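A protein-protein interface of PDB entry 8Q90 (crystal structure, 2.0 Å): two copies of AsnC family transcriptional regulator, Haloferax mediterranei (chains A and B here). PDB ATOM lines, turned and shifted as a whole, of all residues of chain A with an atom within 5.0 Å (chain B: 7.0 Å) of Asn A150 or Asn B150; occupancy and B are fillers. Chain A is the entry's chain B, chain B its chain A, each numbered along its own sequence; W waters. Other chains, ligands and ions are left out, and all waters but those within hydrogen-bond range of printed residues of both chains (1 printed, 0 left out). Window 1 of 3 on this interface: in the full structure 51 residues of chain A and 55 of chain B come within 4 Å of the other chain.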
ATOM      1  N   ILE A  99      16.538 -26.010   1.064  1.00  0.00           N
ATOM      2  CA  ILE A  99      16.054 -25.415  -0.176  1.00  0.00           C
ATOM      3  C   ILE A  99      16.019 -23.883  -0.131  1.00  0.00           C
ATOM      4  O   ILE A  99      15.947 -23.250  -1.191  1.00  0.00           O
ATOM      5  CB  ILE A  99      14.657 -25.962  -0.524  1.00  0.00           C
ATOM      6  CG1 ILE A  99      13.644 -25.552   0.540  1.00  0.00           C
ATOM      7  CG2 ILE A  99      14.683 -27.494  -0.663  1.00  0.00           C
ATOM      8  CD1 ILE A  99      12.221 -25.745   0.117  1.00  0.00           C
ATOM      9  N   SER A 100      16.069 -23.262   1.050  1.00  0.00           N
ATOM     10  CA  SER A 100      16.136 -21.810   1.158  1.00  0.00           C
ATOM     11  C   SER A 100      17.102 -21.425   2.268  1.00  0.00           C
ATOM     12  O   SER A 100      17.120 -22.049   3.330  1.00  0.00           O
ATOM     13  CB  SER A 100      14.747 -21.183   1.429  1.00  0.00           C
ATOM     14  OG  SER A 100      13.914 -21.214   0.273  1.00  0.00           O
ATOM     15  N   THR A 148       0.936 -22.381   2.067  1.00  0.00           N
ATOM     16  CA  THR A 148       1.461 -21.889   0.772  1.00  0.00           C
ATOM     17  C   THR A 148       2.988 -22.019   0.806  1.00  0.00           C
ATOM     18  O   THR A 148       3.574 -21.745   1.845  1.00  0.00           O
ATOM     19  CB  THR A 148       0.983 -20.456   0.509  1.00  0.00           C
ATOM     20  OG1 THR A 148      -0.420 -20.389   0.765  1.00  0.00           O
ATOM     21  CG2 THR A 148       1.273 -19.987  -0.898  1.00  0.00           C
ATOM     22  N   GLU A 149       3.588 -22.424  -0.307  1.00  0.00           N
ATOM     23  CA  GLU A 149       5.060 -22.582  -0.382  1.00  0.00           C
ATOM     24  C   GLU A 149       5.595 -22.133  -1.748  1.00  0.00           C
ATOM     25  O   GLU A 149       5.306 -22.798  -2.748  1.00  0.00           O
ATOM     26  CB  GLU A 149       5.444 -24.022  -0.036  1.00  0.00           C
ATOM     27  CG  GLU A 149       6.902 -24.205   0.335  1.00  0.00           C
ATOM     28  CD  GLU A 149       7.209 -25.538   0.999  1.00  0.00           C
ATOM     29  OE1 GLU A 149       6.517 -26.524   0.685  1.00  0.00           O
ATOM     30  OE2 GLU A 149       8.136 -25.589   1.822  1.00  0.00           O
ATOM     31  N   ASN A 150       6.373 -21.057  -1.760  1.00  0.00           N
ATOM     32  CA  ASN A 150       6.977 -20.518  -3.011  1.00  0.00           C
ATOM     33  C   ASN A 150       5.893 -20.346  -4.087  1.00  0.00           C
ATOM     34  O   ASN A 150       6.139 -20.725  -5.225  1.00  0.00           O
ATOM     35  CB  ASN A 150       8.236 -21.311  -3.386  1.00  0.00           C
ATOM     36  CG  ASN A 150       9.333 -21.167  -2.348  1.00  0.00           C
ATOM     37  OD1 ASN A 150       9.882 -20.086  -2.156  1.00  0.00           O
ATOM     38  ND2 ASN A 150       9.661 -22.247  -1.662  1.00  0.00           N
ATOM     39  N   GLU A 151       4.750 -19.762  -3.724  1.00  0.00           N
ATOM     40  CA  GLU A 151       3.654 -19.491  -4.690  1.00  0.00           C
ATOM     41  C   GLU A 151       3.884 -18.125  -5.333  1.00  0.00           C
ATOM     42  O   GLU A 151       3.520 -17.117  -4.733  1.00  0.00           O
ATOM     43  CB  GLU A 151       2.278 -19.575  -4.031  1.00  0.00           C
ATOM     44  CG  GLU A 151       1.135 -19.659  -5.020  1.00  0.00           C
ATOM     45  CD  GLU A 151       1.104 -20.911  -5.880  1.00  0.00           C
ATOM     46  OE1 GLU A 151       1.870 -21.845  -5.593  1.00  0.00           O
ATOM     47  OE2 GLU A 151       0.307 -20.949  -6.834  1.00  0.00           O
ATOM     48  N   GLN A 152       4.439 -18.128  -6.538  1.00  0.00           N
ATOM     49  CA  GLN A 152       4.770 -16.867  -7.240  1.00  0.00           C
ATOM     50  C   GLN A 152       3.483 -16.105  -7.570  1.00  0.00           C
ATOM     51  O   GLN A 152       2.536 -16.719  -8.045  1.00  0.00           O
ATOM     52  CB  GLN A 152       5.620 -17.191  -8.466  1.00  0.00           C
ATOM     53  CG  GLN A 152       6.962 -17.829  -8.143  1.00  0.00           C
ATOM     54  CD  GLN A 152       7.748 -18.169  -9.387  1.00  0.00           C
ATOM     55  OE1 GLN A 152       8.860 -17.695  -9.592  1.00  0.00           O
ATOM     56  NE2 GLN A 152       7.167 -19.002 -10.234  1.00  0.00           N
ATOM     57  N   THR B  60       6.448 -24.385 -13.742  1.00  0.00           N
ATOM     58  CA  THR B  60       6.414 -22.912 -13.602  1.00  0.00           C
ATOM     59  C   THR B  60       7.747 -22.272 -13.979  1.00  0.00           C
ATOM     60  O   THR B  60       8.788 -22.924 -13.857  1.00  0.00           O
ATOM     61  CB  THR B  60       6.026 -22.520 -12.175  1.00  0.00           C
ATOM     62  OG1 THR B  60       5.548 -21.177 -12.179  1.00  0.00           O
ATOM     63  CG2 THR B  60       7.170 -22.658 -11.196  1.00  0.00           C
ATOM     64  N   ARG B  62      10.889 -19.721 -13.263  1.00  0.00           N
ATOM     65  CA  ARG B  62      11.515 -19.095 -12.076  1.00  0.00           C
ATOM     66  C   ARG B  62      11.620 -17.603 -12.368  1.00  0.00           C
ATOM     67  O   ARG B  62      12.507 -17.223 -13.128  1.00  0.00           O
ATOM     68  CB  ARG B  62      12.884 -19.701 -11.782  1.00  0.00           C
ATOM     69  CG  ARG B  62      13.509 -19.220 -10.485  1.00  0.00           C
ATOM     70  CD  ARG B  62      14.761 -20.026 -10.204  1.00  0.00           C
ATOM     71  NE  ARG B  62      15.466 -19.453  -9.072  1.00  0.00           N
ATOM     72  CZ  ARG B  62      15.259 -19.809  -7.815  1.00  0.00           C
ATOM     73  NH1 ARG B  62      14.378 -20.752  -7.535  1.00  0.00           N
ATOM     74  NH2 ARG B  62      15.942 -19.227  -6.846  1.00  0.00           N
ATOM     75  N   ILE B  99       4.559 -15.160  -0.398  1.00  0.00           N
ATOM     76  CA  ILE B  99       4.762 -16.300  -1.292  1.00  0.00           C
ATOM     77  C   ILE B  99       4.853 -17.633  -0.549  1.00  0.00           C
ATOM     78  O   ILE B  99       4.657 -18.693  -1.169  1.00  0.00           O
ATOM     79  CB  ILE B  99       5.997 -16.057  -2.165  1.00  0.00           C
ATOM     80  CG1 ILE B  99       7.224 -15.869  -1.284  1.00  0.00           C
ATOM     81  CG2 ILE B  99       5.782 -14.805  -3.080  1.00  0.00           C
ATOM     82  CD1 ILE B  99       8.541 -15.929  -2.029  1.00  0.00           C
ATOM     83  N   SER B 100       5.115 -17.611   0.760  1.00  0.00           N
ATOM     84  CA  SER B 100       5.105 -18.802   1.602  1.00  0.00           C
ATOM     85  C   SER B 100       4.387 -18.483   2.903  1.00  0.00           C
ATOM     86  O   SER B 100       4.535 -17.383   3.431  1.00  0.00           O
ATOM     87  CB  SER B 100       6.531 -19.288   1.904  1.00  0.00           C
ATOM     88  OG  SER B 100       7.173 -19.716   0.711  1.00  0.00           O
ATOM     89  N   VAL B 101       3.594 -19.436   3.401  1.00  0.00           N
ATOM     90  CA  VAL B 101       2.872 -19.314   4.668  1.00  0.00           C
ATOM     91  C   VAL B 101       2.893 -20.677   5.348  1.00  0.00           C
ATOM     92  O   VAL B 101       2.387 -21.659   4.792  1.00  0.00           O
ATOM     93  CB  VAL B 101       1.411 -18.843   4.491  1.00  0.00           C
ATOM     94  CG1 VAL B 101       0.760 -18.686   5.846  1.00  0.00           C
ATOM     95  CG2 VAL B 101       1.322 -17.523   3.720  1.00  0.00           C
ATOM     96  N   TYR B 102       3.461 -20.744   6.552  1.00  0.00           N
ATOM     97  CA  TYR B 102       3.645 -21.997   7.267  1.00  0.00           C
ATOM     98  C   TYR B 102       3.019 -21.896   8.645  1.00  0.00           C
ATOM     99  O   TYR B 102       3.291 -20.933   9.370  1.00  0.00           O
ATOM    100  CB  TYR B 102       5.129 -22.333   7.447  1.00  0.00           C
ATOM    101  CG  TYR B 102       5.959 -22.526   6.199  1.00  0.00           C
ATOM    102  CD1 TYR B 102       5.867 -23.688   5.458  1.00  0.00           C
ATOM    103  CD2 TYR B 102       6.898 -21.575   5.815  1.00  0.00           C
ATOM    104  CE1 TYR B 102       6.664 -23.886   4.332  1.00  0.00           C
ATOM    105  CE2 TYR B 102       7.695 -21.754   4.687  1.00  0.00           C
ATOM    106  CZ  TYR B 102       7.577 -22.916   3.950  1.00  0.00           C
ATOM    107  OH  TYR B 102       8.376 -23.103   2.840  1.00  0.00           O
ATOM    108  N   ILE B 113       6.644 -15.548   4.313  1.00  0.00           N
ATOM    109  CA  ILE B 113       7.686 -14.897   3.533  1.00  0.00           C
ATOM    110  C   ILE B 113       7.001 -14.021   2.499  1.00  0.00           C
ATOM    111  O   ILE B 113       6.168 -14.508   1.728  1.00  0.00           O
ATOM    112  CB  ILE B 113       8.613 -15.915   2.847  1.00  0.00           C
ATOM    113  CG1 ILE B 113       9.312 -16.790   3.880  1.00  0.00           C
ATOM    114  CG2 ILE B 113       9.668 -15.192   2.030  1.00  0.00           C
ATOM    115  CD1 ILE B 113       9.964 -18.016   3.240  1.00  0.00           C
ATOM    116  N   THR B 148      19.989 -18.556  -0.940  1.00  0.00           N
ATOM    117  CA  THR B 148      19.316 -19.612  -1.732  1.00  0.00           C
ATOM    118  C   THR B 148      17.798 -19.456  -1.572  1.00  0.00           C
ATOM    119  O   THR B 148      17.350 -19.240  -0.452  1.00  0.00           O
ATOM    120  CB  THR B 148      19.874 -20.988  -1.352  1.00  0.00           C
ATOM    121  OG1 THR B 148      21.234 -21.023  -1.781  1.00  0.00           O
ATOM    122  CG2 THR B 148      19.094 -22.137  -1.950  1.00  0.00           C
ATOM    123  N   GLU B 149      17.060 -19.556  -2.677  1.00  0.00           N
ATOM    124  CA  GLU B 149      15.580 -19.438  -2.625  1.00  0.00           C
ATOM    125  C   GLU B 149      14.911 -20.545  -3.445  1.00  0.00           C
ATOM    126  O   GLU B 149      15.138 -20.597  -4.646  1.00  0.00           O
ATOM    127  CB  GLU B 149      15.117 -18.045  -3.043  1.00  0.00           C
ATOM    128  CG  GLU B 149      13.755 -17.677  -2.485  1.00  0.00           C
ATOM    129  CD  GLU B 149      13.497 -16.189  -2.313  1.00  0.00           C
ATOM    130  OE1 GLU B 149      14.125 -15.393  -3.036  1.00  0.00           O
ATOM    131  OE2 GLU B 149      12.666 -15.835  -1.461  1.00  0.00           O
ATOM    132  N   ASN B 150      14.107 -21.371  -2.786  1.00  0.00           N
ATOM    133  CA  ASN B 150      13.382 -22.495  -3.444  1.00  0.00           C
ATOM    134  C   ASN B 150      14.265 -23.213  -4.468  1.00  0.00           C
ATOM    135  O   ASN B 150      13.843 -23.338  -5.613  1.00  0.00           O
ATOM    136  CB  ASN B 150      12.059 -22.058  -4.073  1.00  0.00           C
ATOM    137  N   GLU B 151      15.456 -23.627  -4.061  1.00  0.00           N
ATOM    138  CA  GLU B 151      16.315 -24.423  -4.971  1.00  0.00           C
ATOM    139  C   GLU B 151      15.996 -25.901  -4.721  1.00  0.00           C
ATOM    140  O   GLU B 151      16.517 -26.470  -3.759  1.00  0.00           O
ATOM    141  CB  GLU B 151      17.783 -24.040  -4.806  1.00  0.00           C
ATOM    142  N   GLN B 152      15.099 -26.449  -5.527  1.00  0.00           N
ATOM    143  CA  GLN B 152      14.698 -27.869  -5.408  1.00  0.00           C
ATOM    144  C   GLN B 152      15.919 -28.762  -5.624  1.00  0.00           C
ATOM    145  O   GLN B 152      16.743 -28.421  -6.474  1.00  0.00           O
ATOM    146  CB  GLN B 152      13.590 -28.139  -6.423  1.00  0.00           C
ATOM    147  CG  GLN B 152      12.299 -27.389  -6.150  1.00  0.00           C
ATOM    148  CD  GLN B 152      11.254 -27.760  -7.172  1.00  0.00           C
ATOM    149  OE1 GLN B 152      10.145 -28.163  -6.839  1.00  0.00           O
ATOM    150  NE2 GLN B 152      11.618 -27.636  -8.437  1.00  0.00           N
ATOM    151  N   PHE B 153      16.018 -29.851  -4.871  1.00  0.00           N
ATOM    152  CA  PHE B 153      17.222 -30.701  -4.947  1.00  0.00           C
ATOM    153  C   PHE B 153      16.982 -31.935  -5.812  1.00  0.00           C
ATOM    154  O   PHE B 153      15.851 -32.389  -5.949  1.00  0.00           O
ATOM    155  CB  PHE B 153      17.665 -31.139  -3.553  1.00  0.00           C
ATOM    156  CG  PHE B 153      16.602 -31.770  -2.693  1.00  0.00           C
ATOM    157  CD1 PHE B 153      15.797 -30.997  -1.874  1.00  0.00           C
ATOM    158  CD2 PHE B 153      16.426 -33.143  -2.678  1.00  0.00           C
ATOM    159  CE1 PHE B 153      14.829 -31.581  -1.076  1.00  0.00           C
ATOM    160  CE2 PHE B 153      15.458 -33.725  -1.876  1.00  0.00           C
ATOM    161  CZ  PHE B 153      14.665 -32.944  -1.074  1.00  0.00           C
HETATM  162  O   HOH W   1       9.388 -20.977   1.506  1.00  0.00           O
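N of Ile B99 sits at hydrogen-bond distance from O of Ile B113, at 2.7 Å.
The guanidinium group of Arg B62 is in hydrogen-bond range of the backbone carbonyl oxygen of Glu B149 (2.7 Å).
The guanidinium group (NH1) of Arg B62 lies within hydrogen-bond range of the backbone carbonyl oxygen (O) of Asn B150.
The backbone carbonyl oxygen (O) of Ser B100 lies within hydrogen-bond range of the backbone NH (N) of Ile B113.
N of Glu B151 is in hydrogen-bond range of O of Ile A99 (2.9 Å).
The backbone NH of Asn B150 is in hydrogen-bond range of the backbone carbonyl oxygen of Ile A99.
N of Glu A151 is in hydrogen-bond range of O of Ile B99, at 2.8 Å.
OG1 of Thr B60 lies within hydrogen-bond range of NE2 of Gln A152 (3.3 Å).
OG of Ser B100 lies within hydrogen-bond range of N of Asn A150 (2.9 Å).
The backbone carbonyl oxygen of Thr A148 lies within hydrogen-bond range of the backbone NH of Val B101 (2.8 Å).
The backbone NH (N) of Asn A150 lies within hydrogen-bond range of the backbone carbonyl oxygen (O) of Ile B99, at 3.0 Å.
The side-chain carboxylate (OE2) of Glu A149 is in hydrogen-bond range of the side-chain hydroxyl (OH) of Tyr B102 (2.7 Å).
N of Asn B150 is in hydrogen-bond range of OG of Ser A100 (3.1 Å).
Printed residues of chain B within 4 Å of Glu A149: Ile B99 (3.6 Å), Ser B100 (3.7 Å) and Tyr B102 (2.7 Å).
Of chain B, only Ile B99, Ser B100 and Asn B150 come within 4 Å of Asn A150.
Of the printed residues of chain B, Gln A152 touches Thr B60 (3.3 Å) and Arg B62 (3.9 Å).
Of the printed residues of chain A, Tyr B102 touches Glu A149 (2.7 Å).
Ile B113 touches none of the printed residues of chain A.
Gln B152 touches none of the printed residues of chain A.
The nearest residue of chain B that does not touch Asn A150 is Glu B149 (4.6 Å).
Ile A99 touches Thr B148, and with the chains exchanged Thr A148 touches Ile B99.
Ile A99 touches Asn B150, and with the chains exchanged Asn A150 touches Ile B99.
Ser A100 touches Thr B148, and with the chains exchanged Thr A148 touches Ser B100.
Asn A150 touches its own counterpart, Asn B150.
7 positions are printed for both chains.
Of the 20 pairs that touch across the chains among the printed residues, 15 have their exchanged pair printed and touching as well.
Water W1 lies within hydrogen-bond range of the side-chain hydroxyl of Ser B100 (2.7 Å), the side-chain hydroxyl of Tyr B102 (2.7 Å) and the side-chain amide nitrogen of Asn A150 (3.4 Å).
Among the printed residues, merely in contact across the chains: Ser A100 with Thr B148 (3.3 Å), Thr A148 with Ser B100 (3.3 Å), Asn A150 with Asn B150 (3.3 Å), Ile A99 with Thr B148 (3.4 Å), Glu A149 with Ile B99 (3.6 Å), Thr A148 with Ile B99 (3.6 Å), Ile A99 with Glu B149 (3.7 Å), Glu A149 with Ser B100 (3.7 Å), Ser A100 with Glu B149 (3.8 Å), Ile A99 with Phe B153 (3.9 Å) and Gln A152 with Arg B62 (3.9 Å).
Printed residues of chain A that touch a printed residue of chain B: Ile A99, Ser A100, Thr A148, Glu A149, Asn A150, Glu A151 and Gln A152.
Hydrophobic or aromatic side chains of chain A within 4 Å of the printed part of chain B: Ile A99.
Of the 13 printed residues of chain B, 11 touch a printed residue of chain A.
Printed residues of chain B that touch a printed residue of chain A: Thr B60, Arg B62, Ile B99, Ser B100, Val B101, Tyr B102, Thr B148, Glu B149, Asn B150, Glu B151 and Phe B153.
Hydrophobic or aromatic side chains of chain B that line the printed part of chain A: Ile B99, Tyr B102 and Phe B153.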
